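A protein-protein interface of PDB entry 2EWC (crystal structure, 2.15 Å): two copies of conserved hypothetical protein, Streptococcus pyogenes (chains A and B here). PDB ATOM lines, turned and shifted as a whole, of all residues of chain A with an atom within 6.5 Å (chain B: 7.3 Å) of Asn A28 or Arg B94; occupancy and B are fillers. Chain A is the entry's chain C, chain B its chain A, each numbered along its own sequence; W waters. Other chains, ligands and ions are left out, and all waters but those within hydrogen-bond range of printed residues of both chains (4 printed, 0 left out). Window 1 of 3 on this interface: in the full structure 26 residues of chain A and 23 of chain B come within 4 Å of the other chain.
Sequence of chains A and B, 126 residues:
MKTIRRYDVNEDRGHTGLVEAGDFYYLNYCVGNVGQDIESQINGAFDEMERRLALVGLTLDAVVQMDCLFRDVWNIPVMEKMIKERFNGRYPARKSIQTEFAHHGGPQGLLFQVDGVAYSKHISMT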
ATOM      1  N   ARG A  13     -30.785  24.657 -27.842  1.00  0.00           N
ATOM      2  CA  ARG A  13     -29.652  24.758 -26.963  1.00  0.00           C
ATOM      3  C   ARG A  13     -29.089  23.367 -26.616  1.00  0.00           C
ATOM      4  O   ARG A  13     -27.957  23.235 -26.092  1.00  0.00           O
ATOM      5  CB  ARG A  13     -30.116  25.501 -25.723  1.00  0.00           C
ATOM      6  CG  ARG A  13     -29.189  26.578 -25.219  1.00  0.00           C
ATOM      7  CD  ARG A  13     -29.314  27.882 -25.968  1.00  0.00           C
ATOM      8  NE  ARG A  13     -28.786  27.769 -27.322  1.00  0.00           N
ATOM      9  CZ  ARG A  13     -29.319  28.367 -28.385  1.00  0.00           C
ATOM     10  NH1 ARG A  13     -30.416  29.126 -28.276  1.00  0.00           N
ATOM     11  NH2 ARG A  13     -28.768  28.181 -29.571  1.00  0.00           N
ATOM     12  N   GLY A  14     -29.860  22.328 -26.933  1.00  0.00           N
ATOM     13  CA  GLY A  14     -29.535  20.951 -26.549  1.00  0.00           C
ATOM     14  C   GLY A  14     -29.316  20.746 -25.045  1.00  0.00           C
ATOM     15  O   GLY A  14     -28.315  20.153 -24.622  1.00  0.00           O
ATOM     16  N   HIS A  15     -30.239  21.241 -24.221  1.00  0.00           N
ATOM     17  CA  HIS A  15     -30.194  20.903 -22.816  1.00  0.00           C
ATOM     18  C   HIS A  15     -31.588  20.660 -22.249  1.00  0.00           C
ATOM     19  O   HIS A  15     -32.591  20.991 -22.878  1.00  0.00           O
ATOM     20  CB  HIS A  15     -29.424  21.943 -22.006  1.00  0.00           C
ATOM     21  CG  HIS A  15     -29.980  23.321 -22.086  1.00  0.00           C
ATOM     22  ND1 HIS A  15     -31.301  23.614 -21.827  1.00  0.00           N
ATOM     23  CD2 HIS A  15     -29.381  24.504 -22.346  1.00  0.00           C
ATOM     24  CE1 HIS A  15     -31.501  24.912 -21.961  1.00  0.00           C
ATOM     25  NE2 HIS A  15     -30.353  25.475 -22.280  1.00  0.00           N
ATOM     26  N   THR A  16     -31.621  20.098 -21.048  1.00  0.00           N
ATOM     27  CA  THR A  16     -32.865  19.868 -20.319  1.00  0.00           C
ATOM     28  C   THR A  16     -32.854  20.781 -19.105  1.00  0.00           C
ATOM     29  O   THR A  16     -31.877  20.818 -18.334  1.00  0.00           O
ATOM     30  CB  THR A  16     -33.015  18.362 -19.952  1.00  0.00           C
ATOM     31  OG1 THR A  16     -33.129  17.625 -21.170  1.00  0.00           O
ATOM     32  CG2 THR A  16     -34.232  18.083 -19.081  1.00  0.00           C
ATOM     33  N   GLY A  17     -33.940  21.541 -18.956  1.00  0.00           N
ATOM     34  CA  GLY A  17     -34.039  22.477 -17.852  1.00  0.00           C
ATOM     35  C   GLY A  17     -34.046  21.783 -16.502  1.00  0.00           C
ATOM     36  O   GLY A  17     -33.487  22.289 -15.545  1.00  0.00           O
ATOM     37  N   LEU A  18     -34.720  20.631 -16.420  1.00  0.00           N
ATOM     38  CA  LEU A  18     -34.824  19.894 -15.178  1.00  0.00           C
ATOM     39  C   LEU A  18     -34.901  18.416 -15.481  1.00  0.00           C
ATOM     40  O   LEU A  18     -35.848  17.964 -16.142  1.00  0.00           O
ATOM     41  CB  LEU A  18     -36.080  20.309 -14.397  1.00  0.00           C
ATOM     42  CG  LEU A  18     -36.324  19.501 -13.103  1.00  0.00           C
ATOM     43  CD1 LEU A  18     -35.474  20.021 -11.983  1.00  0.00           C
ATOM     44  CD2 LEU A  18     -37.756  19.602 -12.681  1.00  0.00           C
ATOM     45  N   VAL A  19     -33.940  17.667 -14.953  1.00  0.00           N
ATOM     46  CA  VAL A  19     -33.876  16.233 -15.142  1.00  0.00           C
ATOM     47  C   VAL A  19     -34.215  15.544 -13.831  1.00  0.00           C
ATOM     48  O   VAL A  19     -33.560  15.774 -12.832  1.00  0.00           O
ATOM     49  CB  VAL A  19     -32.469  15.772 -15.597  1.00  0.00           C
ATOM     50  CG1 VAL A  19     -32.444  14.245 -15.810  1.00  0.00           C
ATOM     51  CG2 VAL A  19     -32.074  16.461 -16.877  1.00  0.00           C
ATOM     52  N   TYR A  26     -31.979  17.519 -11.343  1.00  0.00           N
ATOM     53  CA  TYR A  26     -30.834  18.304 -11.755  1.00  0.00           C
ATOM     54  C   TYR A  26     -31.341  19.437 -12.611  1.00  0.00           C
ATOM     55  O   TYR A  26     -32.020  19.218 -13.598  1.00  0.00           O
ATOM     56  CB  TYR A  26     -29.803  17.437 -12.508  1.00  0.00           C
ATOM     57  CG  TYR A  26     -29.198  16.406 -11.587  1.00  0.00           C
ATOM     58  CD1 TYR A  26     -27.956  16.608 -11.009  1.00  0.00           C
ATOM     59  CD2 TYR A  26     -29.910  15.257 -11.241  1.00  0.00           C
ATOM     60  CE1 TYR A  26     -27.416  15.694 -10.161  1.00  0.00           C
ATOM     61  CE2 TYR A  26     -29.386  14.338 -10.381  1.00  0.00           C
ATOM     62  CZ  TYR A  26     -28.139  14.556  -9.841  1.00  0.00           C
ATOM     63  OH  TYR A  26     -27.606  13.608  -8.973  1.00  0.00           O
ATOM     64  N   LEU A  27     -30.985  20.644 -12.198  1.00  0.00           N
ATOM     65  CA  LEU A  27     -31.373  21.883 -12.837  1.00  0.00           C
ATOM     66  C   LEU A  27     -30.265  22.365 -13.745  1.00  0.00           C
ATOM     67  O   LEU A  27     -29.099  22.439 -13.332  1.00  0.00           O
ATOM     68  CB  LEU A  27     -31.608  22.927 -11.764  1.00  0.00           C
ATOM     69  CG  LEU A  27     -32.875  22.687 -10.959  1.00  0.00           C
ATOM     70  CD1 LEU A  27     -32.756  23.361  -9.608  1.00  0.00           C
ATOM     71  CD2 LEU A  27     -34.033  23.270 -11.730  1.00  0.00           C
ATOM     72  N   ASN A  28     -30.635  22.668 -14.982  1.00  0.00           N
ATOM     73  CA  ASN A  28     -29.769  23.316 -15.938  1.00  0.00           C
ATOM     74  C   ASN A  28     -29.437  24.721 -15.429  1.00  0.00           C
ATOM     75  O   ASN A  28     -30.158  25.230 -14.562  1.00  0.00           O
ATOM     76  CB  ASN A  28     -30.554  23.452 -17.245  1.00  0.00           C
ATOM     77  CG  ASN A  28     -29.697  23.857 -18.410  1.00  0.00           C
ATOM     78  OD1 ASN A  28     -29.748  24.997 -18.880  1.00  0.00           O
ATOM     79  ND2 ASN A  28     -28.902  22.943 -18.878  1.00  0.00           N
ATOM     80  N   TYR A  29     -28.418  25.388 -15.971  1.00  0.00           N
ATOM     81  CA  TYR A  29     -28.198  26.771 -15.538  1.00  0.00           C
ATOM     82  C   TYR A  29     -29.529  27.542 -15.696  1.00  0.00           C
ATOM     83  O   TYR A  29     -30.284  27.324 -16.650  1.00  0.00           O
ATOM     84  CB  TYR A  29     -27.027  27.456 -16.285  1.00  0.00           C
ATOM     85  CG  TYR A  29     -27.298  27.679 -17.750  1.00  0.00           C
ATOM     86  CD1 TYR A  29     -27.959  28.830 -18.190  1.00  0.00           C
ATOM     87  CD2 TYR A  29     -26.918  26.715 -18.705  1.00  0.00           C
ATOM     88  CE1 TYR A  29     -28.239  29.024 -19.553  1.00  0.00           C
ATOM     89  CE2 TYR A  29     -27.182  26.896 -20.080  1.00  0.00           C
ATOM     90  CZ  TYR A  29     -27.843  28.055 -20.488  1.00  0.00           C
ATOM     91  OH  TYR A  29     -28.110  28.249 -21.836  1.00  0.00           O
ATOM     92  N   CYS A  30     -29.822  28.385 -14.721  1.00  0.00           N
ATOM     93  CA  CYS A  30     -30.987  29.250 -14.709  1.00  0.00           C
ATOM     94  C   CYS A  30     -30.543  30.690 -14.802  1.00  0.00           C
ATOM     95  O   CYS A  30     -29.578  31.126 -14.138  1.00  0.00           O
ATOM     96  CB  CYS A  30     -31.772  29.104 -13.408  1.00  0.00           C
ATOM     97  SG  CYS A  30     -32.374  27.450 -13.075  1.00  0.00           S
ATOM     98  N   VAL A  31     -31.310  31.443 -15.567  1.00  0.00           N
ATOM     99  CA  VAL A  31     -31.021  32.822 -15.816  1.00  0.00           C
ATOM    100  C   VAL A  31     -32.341  33.597 -15.880  1.00  0.00           C
ATOM    101  O   VAL A  31     -33.393  33.038 -16.270  1.00  0.00           O
ATOM    102  CB  VAL A  31     -30.214  32.898 -17.133  1.00  0.00           C
ATOM    103  CG1 VAL A  31     -31.086  33.273 -18.317  1.00  0.00           C
ATOM    104  CG2 VAL A  31     -29.092  33.812 -16.985  1.00  0.00           C
ATOM    105  N   GLU A  48     -36.541  31.617 -12.282  1.00  0.00           N
ATOM    106  CA  GLU A  48     -36.426  30.489 -13.215  1.00  0.00           C
ATOM    107  C   GLU A  48     -36.181  29.156 -12.508  1.00  0.00           C
ATOM    108  O   GLU A  48     -36.753  28.156 -12.889  1.00  0.00           O
ATOM    109  CB  GLU A  48     -35.389  30.756 -14.331  1.00  0.00           C
ATOM    110  CG  GLU A  48     -35.001  29.503 -15.151  1.00  0.00           C
ATOM    111  CD  GLU A  48     -34.741  29.764 -16.644  1.00  0.00           C
ATOM    112  OE1 GLU A  48     -33.553  29.988 -17.039  1.00  0.00           O
ATOM    113  OE2 GLU A  48     -35.723  29.715 -17.428  1.00  0.00           O
ATOM    114  N   MET A  49     -35.354  29.141 -11.470  1.00  0.00           N
ATOM    115  CA  MET A  49     -35.157  27.911 -10.676  1.00  0.00           C
ATOM    116  C   MET A  49     -36.508  27.463 -10.082  1.00  0.00           C
ATOM    117  O   MET A  49     -36.859  26.287 -10.156  1.00  0.00           O
ATOM    118  CB  MET A  49     -34.087  28.127  -9.583  1.00  0.00           C
ATOM    119  CG  MET A  49     -33.905  27.012  -8.524  1.00  0.00           C
ATOM    120  SD  MET A  49     -32.477  27.389  -7.417  1.00  0.00           S
ATOM    121  CE  MET A  49     -31.130  26.844  -8.476  1.00  0.00           C
ATOM    122  N   ARG A  52     -38.977  26.116 -12.706  1.00  0.00           N
ATOM    123  CA  ARG A  52     -38.549  24.748 -13.027  1.00  0.00           C
ATOM    124  C   ARG A  52     -38.912  23.774 -11.940  1.00  0.00           C
ATOM    125  O   ARG A  52     -39.463  22.736 -12.236  1.00  0.00           O
ATOM    126  CB  ARG A  52     -37.052  24.669 -13.324  1.00  0.00           C
ATOM    127  CG  ARG A  52     -36.751  24.861 -14.772  1.00  0.00           C
ATOM    128  CD  ARG A  52     -35.346  25.317 -15.000  1.00  0.00           C
ATOM    129  NE  ARG A  52     -35.102  25.527 -16.416  1.00  0.00           N
ATOM    130  CZ  ARG A  52     -33.964  25.995 -16.928  1.00  0.00           C
ATOM    131  NH1 ARG A  52     -32.972  26.346 -16.135  1.00  0.00           N
ATOM    132  NH2 ARG A  52     -33.834  26.136 -18.255  1.00  0.00           N
ATOM    133  N   VAL A 114     -27.246  30.450 -12.155  1.00  0.00           N
ATOM    134  CA  VAL A 114     -27.184  29.507 -11.041  1.00  0.00           C
ATOM    135  C   VAL A 114     -27.726  28.166 -11.526  1.00  0.00           C
ATOM    136  O   VAL A 114     -28.649  28.121 -12.334  1.00  0.00           O
ATOM    137  CB  VAL A 114     -27.957  30.046  -9.778  1.00  0.00           C
ATOM    138  CG1 VAL A 114     -29.461  30.142 -10.050  1.00  0.00           C
ATOM    139  CG2 VAL A 114     -27.688  29.180  -8.547  1.00  0.00           C
ATOM    140  N   ASP A 115     -27.135  27.070 -11.087  1.00  0.00           N
ATOM    141  CA  ASP A 115     -27.736  25.774 -11.365  1.00  0.00           C
ATOM    142  C   ASP A 115     -27.789  25.074 -10.031  1.00  0.00           C
ATOM    143  O   ASP A 115     -27.353  25.629  -9.030  1.00  0.00           O
ATOM    144  CB  ASP A 115     -26.963  25.003 -12.457  1.00  0.00           C
ATOM    145  CG  ASP A 115     -25.705  24.290 -11.932  1.00  0.00           C
ATOM    146  OD1 ASP A 115     -25.084  23.524 -12.709  1.00  0.00           O
ATOM    147  OD2 ASP A 115     -25.333  24.461 -10.749  1.00  0.00           O
ATOM    148  N   GLY A 116     -28.349  23.883  -9.976  1.00  0.00           N
ATOM    149  CA  GLY A 116     -28.465  23.216  -8.675  1.00  0.00           C
ATOM    150  C   GLY A 116     -28.938  21.781  -8.763  1.00  0.00           C
ATOM    151  O   GLY A 116     -29.123  21.230  -9.857  1.00  0.00           O
ATOM    152  N   VAL B  64     -27.400  12.619 -16.736  1.00  0.00           N
ATOM    153  CA  VAL B  64     -28.393  13.578 -16.256  1.00  0.00           C
ATOM    154  C   VAL B  64     -27.899  15.015 -16.121  1.00  0.00           C
ATOM    155  O   VAL B  64     -28.708  15.948 -16.148  1.00  0.00           O
ATOM    156  CB  VAL B  64     -29.069  13.097 -14.926  1.00  0.00           C
ATOM    157  CG1 VAL B  64     -29.806  11.758 -15.171  1.00  0.00           C
ATOM    158  CG2 VAL B  64     -28.087  13.004 -13.782  1.00  0.00           C
ATOM    159  N   GLN B  65     -26.583  15.186 -15.975  1.00  0.00           N
ATOM    160  CA  GLN B  65     -25.985  16.483 -15.710  1.00  0.00           C
ATOM    161  C   GLN B  65     -24.545  16.484 -16.189  1.00  0.00           C
ATOM    162  O   GLN B  65     -23.850  15.490 -16.023  1.00  0.00           O
ATOM    163  CB  GLN B  65     -26.072  16.858 -14.214  1.00  0.00           C
ATOM    164  CG  GLN B  65     -25.849  18.340 -13.948  1.00  0.00           C
ATOM    165  CD  GLN B  65     -24.368  18.687 -13.840  1.00  0.00           C
ATOM    166  OE1 GLN B  65     -23.548  17.832 -13.475  1.00  0.00           O
ATOM    167  NE2 GLN B  65     -24.004  19.925 -14.218  1.00  0.00           N
ATOM    168  N   MET B  66     -24.118  17.583 -16.828  1.00  0.00           N
ATOM    169  CA  MET B  66     -22.727  17.715 -17.299  1.00  0.00           C
ATOM    170  C   MET B  66     -22.224  19.092 -16.944  1.00  0.00           C
ATOM    171  O   MET B  66     -22.949  20.074 -17.121  1.00  0.00           O
ATOM    172  CB  MET B  66     -22.627  17.589 -18.832  1.00  0.00           C
ATOM    173  CG  MET B  66     -23.111  16.309 -19.424  1.00  0.00           C
ATOM    174  SD  MET B  66     -22.509  16.159 -21.148  1.00  0.00           S
ATOM    175  CE  MET B  66     -23.079  17.676 -21.905  1.00  0.00           C
ATOM    176  N   ASP B  67     -20.992  19.178 -16.464  1.00  0.00           N
ATOM    177  CA  ASP B  67     -20.297  20.487 -16.379  1.00  0.00           C
ATOM    178  C   ASP B  67     -19.276  20.573 -17.505  1.00  0.00           C
ATOM    179  O   ASP B  67     -18.424  19.696 -17.623  1.00  0.00           O
ATOM    180  CB  ASP B  67     -19.578  20.641 -15.051  1.00  0.00           C
ATOM    181  CG  ASP B  67     -20.538  20.821 -13.877  1.00  0.00           C
ATOM    182  OD1 ASP B  67     -21.623  21.421 -14.074  1.00  0.00           O
ATOM    183  OD2 ASP B  67     -20.214  20.368 -12.747  1.00  0.00           O
ATOM    184  N   CYS B  68     -19.367  21.619 -18.323  1.00  0.00           N
ATOM    185  CA  CYS B  68     -18.487  21.798 -19.484  1.00  0.00           C
ATOM    186  C   CYS B  68     -17.469  22.939 -19.253  1.00  0.00           C
ATOM    187  O   CYS B  68     -17.837  24.086 -18.933  1.00  0.00           O
ATOM    188  CB  CYS B  68     -19.334  22.093 -20.715  1.00  0.00           C
ATOM    189  SG  CYS B  68     -20.811  21.047 -20.854  1.00  0.00           S
ATOM    190  N   PHE B  70     -14.444  25.199 -20.701  1.00  0.00           N
ATOM    191  CA  PHE B  70     -13.856  25.735 -21.936  1.00  0.00           C
ATOM    192  C   PHE B  70     -12.686  26.632 -21.622  1.00  0.00           C
ATOM    193  O   PHE B  70     -12.694  27.351 -20.631  1.00  0.00           O
ATOM    194  CB  PHE B  70     -14.873  26.586 -22.689  1.00  0.00           C
ATOM    195  CG  PHE B  70     -16.052  25.816 -23.219  1.00  0.00           C
ATOM    196  CD1 PHE B  70     -16.046  25.329 -24.511  1.00  0.00           C
ATOM    197  CD2 PHE B  70     -17.188  25.629 -22.431  1.00  0.00           C
ATOM    198  CE1 PHE B  70     -17.169  24.636 -25.027  1.00  0.00           C
ATOM    199  CE2 PHE B  70     -18.323  24.935 -22.922  1.00  0.00           C
ATOM    200  CZ  PHE B  70     -18.304  24.435 -24.220  1.00  0.00           C
ATOM    201  N   ILE B  76     -19.369  27.567 -26.920  1.00  0.00           N
ATOM    202  CA  ILE B  76     -20.591  26.798 -26.622  1.00  0.00           C
ATOM    203  C   ILE B  76     -21.350  26.345 -27.902  1.00  0.00           C
ATOM    204  O   ILE B  76     -21.749  25.189 -27.967  1.00  0.00           O
ATOM    205  CB  ILE B  76     -21.539  27.501 -25.650  1.00  0.00           C
ATOM    206  CG1 ILE B  76     -21.045  27.343 -24.207  1.00  0.00           C
ATOM    207  CG2 ILE B  76     -22.963  26.894 -25.747  1.00  0.00           C
ATOM    208  CD1 ILE B  76     -21.664  28.399 -23.228  1.00  0.00           C
ATOM    209  N   PRO B  77     -21.561  27.242 -28.901  1.00  0.00           N
ATOM    210  CA  PRO B  77     -22.316  26.768 -30.071  1.00  0.00           C
ATOM    211  C   PRO B  77     -21.704  25.535 -30.700  1.00  0.00           C
ATOM    212  O   PRO B  77     -22.431  24.680 -31.205  1.00  0.00           O
ATOM    213  CB  PRO B  77     -22.251  27.956 -31.042  1.00  0.00           C
ATOM    214  CG  PRO B  77     -22.146  29.154 -30.133  1.00  0.00           C
ATOM    215  CD  PRO B  77     -21.211  28.670 -29.036  1.00  0.00           C
ATOM    216  N   MET B  79     -20.118  23.108 -29.189  1.00  0.00           N
ATOM    217  CA  MET B  79     -20.541  21.981 -28.331  1.00  0.00           C
ATOM    218  C   MET B  79     -22.010  21.604 -28.534  1.00  0.00           C
ATOM    219  O   MET B  79     -22.365  20.415 -28.497  1.00  0.00           O
ATOM    220  CB  MET B  79     -20.299  22.288 -26.833  1.00  0.00           C
ATOM    221  CG  MET B  79     -20.565  21.066 -25.892  1.00  0.00           C
ATOM    222  SD  MET B  79     -20.617  21.359 -24.095  1.00  0.00           S
ATOM    223  CE  MET B  79     -21.882  22.640 -24.035  1.00  0.00           C
ATOM    224  N   GLU B  80     -22.860  22.615 -28.725  1.00  0.00           N
ATOM    225  CA  GLU B  80     -24.295  22.408 -28.916  1.00  0.00           C
ATOM    226  C   GLU B  80     -24.573  21.613 -30.177  1.00  0.00           C
ATOM    227  O   GLU B  80     -25.396  20.716 -30.173  1.00  0.00           O
ATOM    228  CB  GLU B  80     -25.032  23.737 -29.003  1.00  0.00           C
ATOM    229  CG  GLU B  80     -25.187  24.414 -27.665  1.00  0.00           C
ATOM    230  CD  GLU B  80     -25.983  25.705 -27.757  1.00  0.00           C
ATOM    231  OE1 GLU B  80     -26.229  26.196 -28.887  1.00  0.00           O
ATOM    232  OE2 GLU B  80     -26.374  26.227 -26.693  1.00  0.00           O
ATOM    233  N   ILE B  83     -23.586  17.993 -29.329  1.00  0.00           N
ATOM    234  CA  ILE B  83     -24.582  17.407 -28.443  1.00  0.00           C
ATOM    235  C   ILE B  83     -25.812  16.980 -29.257  1.00  0.00           C
ATOM    236  O   ILE B  83     -26.314  15.870 -29.089  1.00  0.00           O
ATOM    237  CB  ILE B  83     -24.977  18.364 -27.280  1.00  0.00           C
ATOM    238  CG1 ILE B  83     -23.862  18.436 -26.237  1.00  0.00           C
ATOM    239  CG2 ILE B  83     -26.238  17.896 -26.568  1.00  0.00           C
ATOM    240  CD1 ILE B  83     -24.019  19.598 -25.261  1.00  0.00           C
ATOM    241  N   TYR B  91     -31.200  15.111 -23.654  1.00  0.00           N
ATOM    242  CA  TYR B  91     -30.142  16.010 -23.175  1.00  0.00           C
ATOM    243  C   TYR B  91     -30.033  16.065 -21.665  1.00  0.00           C
ATOM    244  O   TYR B  91     -31.041  16.019 -20.962  1.00  0.00           O
ATOM    245  CB  TYR B  91     -30.341  17.423 -23.716  1.00  0.00           C
ATOM    246  CG  TYR B  91     -30.626  17.454 -25.205  1.00  0.00           C
ATOM    247  CD1 TYR B  91     -29.728  16.878 -26.114  1.00  0.00           C
ATOM    248  CD2 TYR B  91     -31.795  18.037 -25.701  1.00  0.00           C
ATOM    249  CE1 TYR B  91     -29.998  16.867 -27.478  1.00  0.00           C
ATOM    250  CE2 TYR B  91     -32.073  18.055 -27.091  1.00  0.00           C
ATOM    251  CZ  TYR B  91     -31.165  17.459 -27.964  1.00  0.00           C
ATOM    252  OH  TYR B  91     -31.408  17.435 -29.322  1.00  0.00           O
ATOM    253  N   PRO B  92     -28.797  16.175 -21.155  1.00  0.00           N
ATOM    254  CA  PRO B  92     -28.607  16.480 -19.735  1.00  0.00           C
ATOM    255  C   PRO B  92     -28.872  17.953 -19.375  1.00  0.00           C
ATOM    256  O   PRO B  92     -28.902  18.822 -20.271  1.00  0.00           O
ATOM    257  CB  PRO B  92     -27.125  16.129 -19.498  1.00  0.00           C
ATOM    258  CG  PRO B  92     -26.478  16.303 -20.824  1.00  0.00           C
ATOM    259  CD  PRO B  92     -27.518  15.950 -21.858  1.00  0.00           C
ATOM    260  N   ALA B  93     -29.117  18.203 -18.083  1.00  0.00           N
ATOM    261  CA  ALA B  93     -28.943  19.528 -17.486  1.00  0.00           C
ATOM    262  C   ALA B  93     -27.433  19.875 -17.537  1.00  0.00           C
ATOM    263  O   ALA B  93     -26.577  18.980 -17.382  1.00  0.00           O
ATOM    264  CB  ALA B  93     -29.431  19.527 -16.031  1.00  0.00           C
ATOM    265  N   ARG B  94     -27.102  21.146 -17.766  1.00  0.00           N
ATOM    266  CA  ARG B  94     -25.699  21.515 -17.822  1.00  0.00           C
ATOM    267  C   ARG B  94     -25.382  22.934 -17.372  1.00  0.00           C
ATOM    268  O   ARG B  94     -26.258  23.792 -17.241  1.00  0.00           O
ATOM    269  CB  ARG B  94     -25.114  21.267 -19.239  1.00  0.00           C
ATOM    270  CG  ARG B  94     -25.485  22.304 -20.259  1.00  0.00           C
ATOM    271  CD  ARG B  94     -24.603  22.233 -21.547  1.00  0.00           C
ATOM    272  NE  ARG B  94     -24.929  23.371 -22.410  1.00  0.00           N
ATOM    273  CZ  ARG B  94     -25.746  23.320 -23.458  1.00  0.00           C
ATOM    274  NH1 ARG B  94     -26.003  24.434 -24.141  1.00  0.00           N
ATOM    275  NH2 ARG B  94     -26.285  22.159 -23.843  1.00  0.00           N
ATOM    276  N   LYS B  95     -24.105  23.161 -17.120  1.00  0.00           N
ATOM    277  CA  LYS B  95     -23.606  24.498 -17.118  1.00  0.00           C
ATOM    278  C   LYS B  95     -22.248  24.512 -17.804  1.00  0.00           C
ATOM    279  O   LYS B  95     -21.548  23.499 -17.827  1.00  0.00           O
ATOM    280  CB  LYS B  95     -23.556  25.057 -15.695  1.00  0.00           C
ATOM    281  CG  LYS B  95     -22.509  24.409 -14.831  1.00  0.00           C
ATOM    282  CD  LYS B  95     -22.399  25.146 -13.493  1.00  0.00           C
ATOM    283  CE  LYS B  95     -21.564  24.330 -12.520  1.00  0.00           C
ATOM    284  NZ  LYS B  95     -22.409  23.208 -12.127  1.00  0.00           N
ATOM    285  N   SER B  96     -21.903  25.660 -18.369  1.00  0.00           N
ATOM    286  CA  SER B  96     -20.590  25.895 -18.945  1.00  0.00           C
ATOM    287  C   SER B  96     -19.781  26.971 -18.174  1.00  0.00           C
ATOM    288  O   SER B  96     -20.327  27.981 -17.710  1.00  0.00           O
ATOM    289  CB  SER B  96     -20.755  26.303 -20.404  1.00  0.00           C
ATOM    290  OG  SER B  96     -21.471  25.298 -21.099  1.00  0.00           O
HETATM  291  O   HOH W   1     -25.682  27.435 -23.350  1.00  0.00           O
HETATM  292  O   HOH W   2     -26.403  21.863 -14.259  1.00  0.00           O
HETATM  293  O   HOH W   3     -26.975  19.596 -22.259  1.00  0.00           O
HETATM  294  O   HOH W   4     -33.861  16.139 -23.487  1.00  0.00           O
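Of chain B, only Ala B93 and Arg B94 come within 4 Å of Asn A28.
Arg B94 touches just these residues of chain A: Arg A13, Gly A14, His A15, Asn A28 and Tyr A29.
Printed residues of chain B within 4 Å of His A15: Tyr B91, Pro B92 and Arg B94.
Printed residues of chain A within 4 Å of Tyr B91: Gly A14 (3.5 Å), His A15 (3.6 Å) and Thr A16 (2.6 Å).
Printed residues of chain B within 4 Å of Tyr A29: Arg B94 (3.0 Å).
Cys B68 touches none of the printed residues of chain A.
The nearest residue of chain B that does not touch Asn A28 is Pro B92 (4.4 Å).
O of Met B66 is in hydrogen-bond range of N of Lys B95, 3.3 Å away.
NE2 of Gln B65 sits at hydrogen-bond distance from OD1 of Asp B67, at 2.8 Å.
The side-chain carboxylate (OE2) of Glu B80 lies within salt-bridge range of the guanidinium group (NH1) of Arg B94 (3.1 Å).
The backbone carbonyl oxygen (O) of Gly A116 is in hydrogen-bond range of the backbone NH (N) of Leu A27 (3.0 Å).
The backbone NH of Cys B68 is in hydrogen-bond range of the backbone carbonyl oxygen of Lys B95 (2.9 Å).
NE2 of His A15 sits at hydrogen-bond distance from OD1 of Asn A28, at 3.5 Å.
Among the printed residues, pairs that only touch across the chains: Thr A16 with Ala B93, Val A19 with Val B64, Gly A14 with Tyr B91, Asn A28 with Ala B93, His A15 with Pro B92, Tyr A26 with Ala B93, His A15 with Tyr B91, Gly A14 with Ile B83, Val A19 with Ala B93, His A15 with Arg B94, Tyr A26 with Gln B65, Leu A27 with Ala B93 and Tyr A26 with Val B64.
No position is printed for both chains.
Of the 21 pairs that touch across the chains among the printed residues, none has its exchanged pair printed and touching as well.
NE of Arg A13 is in salt-bridge range of OE2 of Glu B80.
O of Pro B92 lies within hydrogen-bond range of N of Thr A16 (3.1 Å).
N of Tyr A29 sits at hydrogen-bond distance from O of Arg B94.
NH2 of Arg B94 lies within hydrogen-bond range of O of Gly A14 (3.0 Å).
The side-chain amino group of Lys B95 is in salt-bridge range of the side-chain carboxylate of Asp A115 (2.8 Å).
N of Arg B94 sits close to ND2 of Asn A28 (2.8 Å).
The side-chain hydroxyl of Thr A16 is in hydrogen-bond range of the backbone carbonyl oxygen of Tyr B91, at 2.6 Å.
O of Arg A13 sits at hydrogen-bond distance from NH2 of Arg B94 (3.0 Å).
Hydrophobic or aromatic side chains of chain A within 4 Å of the printed part of chain B: His A15, Val A19, Tyr A26 and Tyr A29.
Hydrophobic or aromatic side chains of chain B that line the printed part of chain A: Val B64, Ile B83, Tyr B91 and Ala B93.
Along chain B the printed residues that touch a printed residue of chain A span positions 64 to 95.
Among the printed residues, 21 pairs touch across the chains.
Among the printed residues, Asp or Glu carboxylates within 4 Å of a Lys or Arg side-chain nitrogen of the other chain: Arg A13 with Glu B80 (2.9 Å) and Asp A115 with Lys B95 (2.8 Å).
Water W2 lies within hydrogen-bond range of OD1 of Asp A115 (2.6 Å), O of Leu A27 (2.9 Å) and NE2 of Gln B65 (3.1 Å).
Water W3 lies within hydrogen-bond range of O of Gly A14 (2.8 Å), O of Pro B92 (2.9 Å) and NH2 of Arg B94 (3.1 Å).
Water W4 lies within hydrogen-bond range of the side-chain hydroxyl (OG1) of Thr A16 and the backbone NH (N) of Tyr B91.
Water W1 lies within hydrogen-bond range of OH of Tyr A29 and NH1 of Arg B94.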
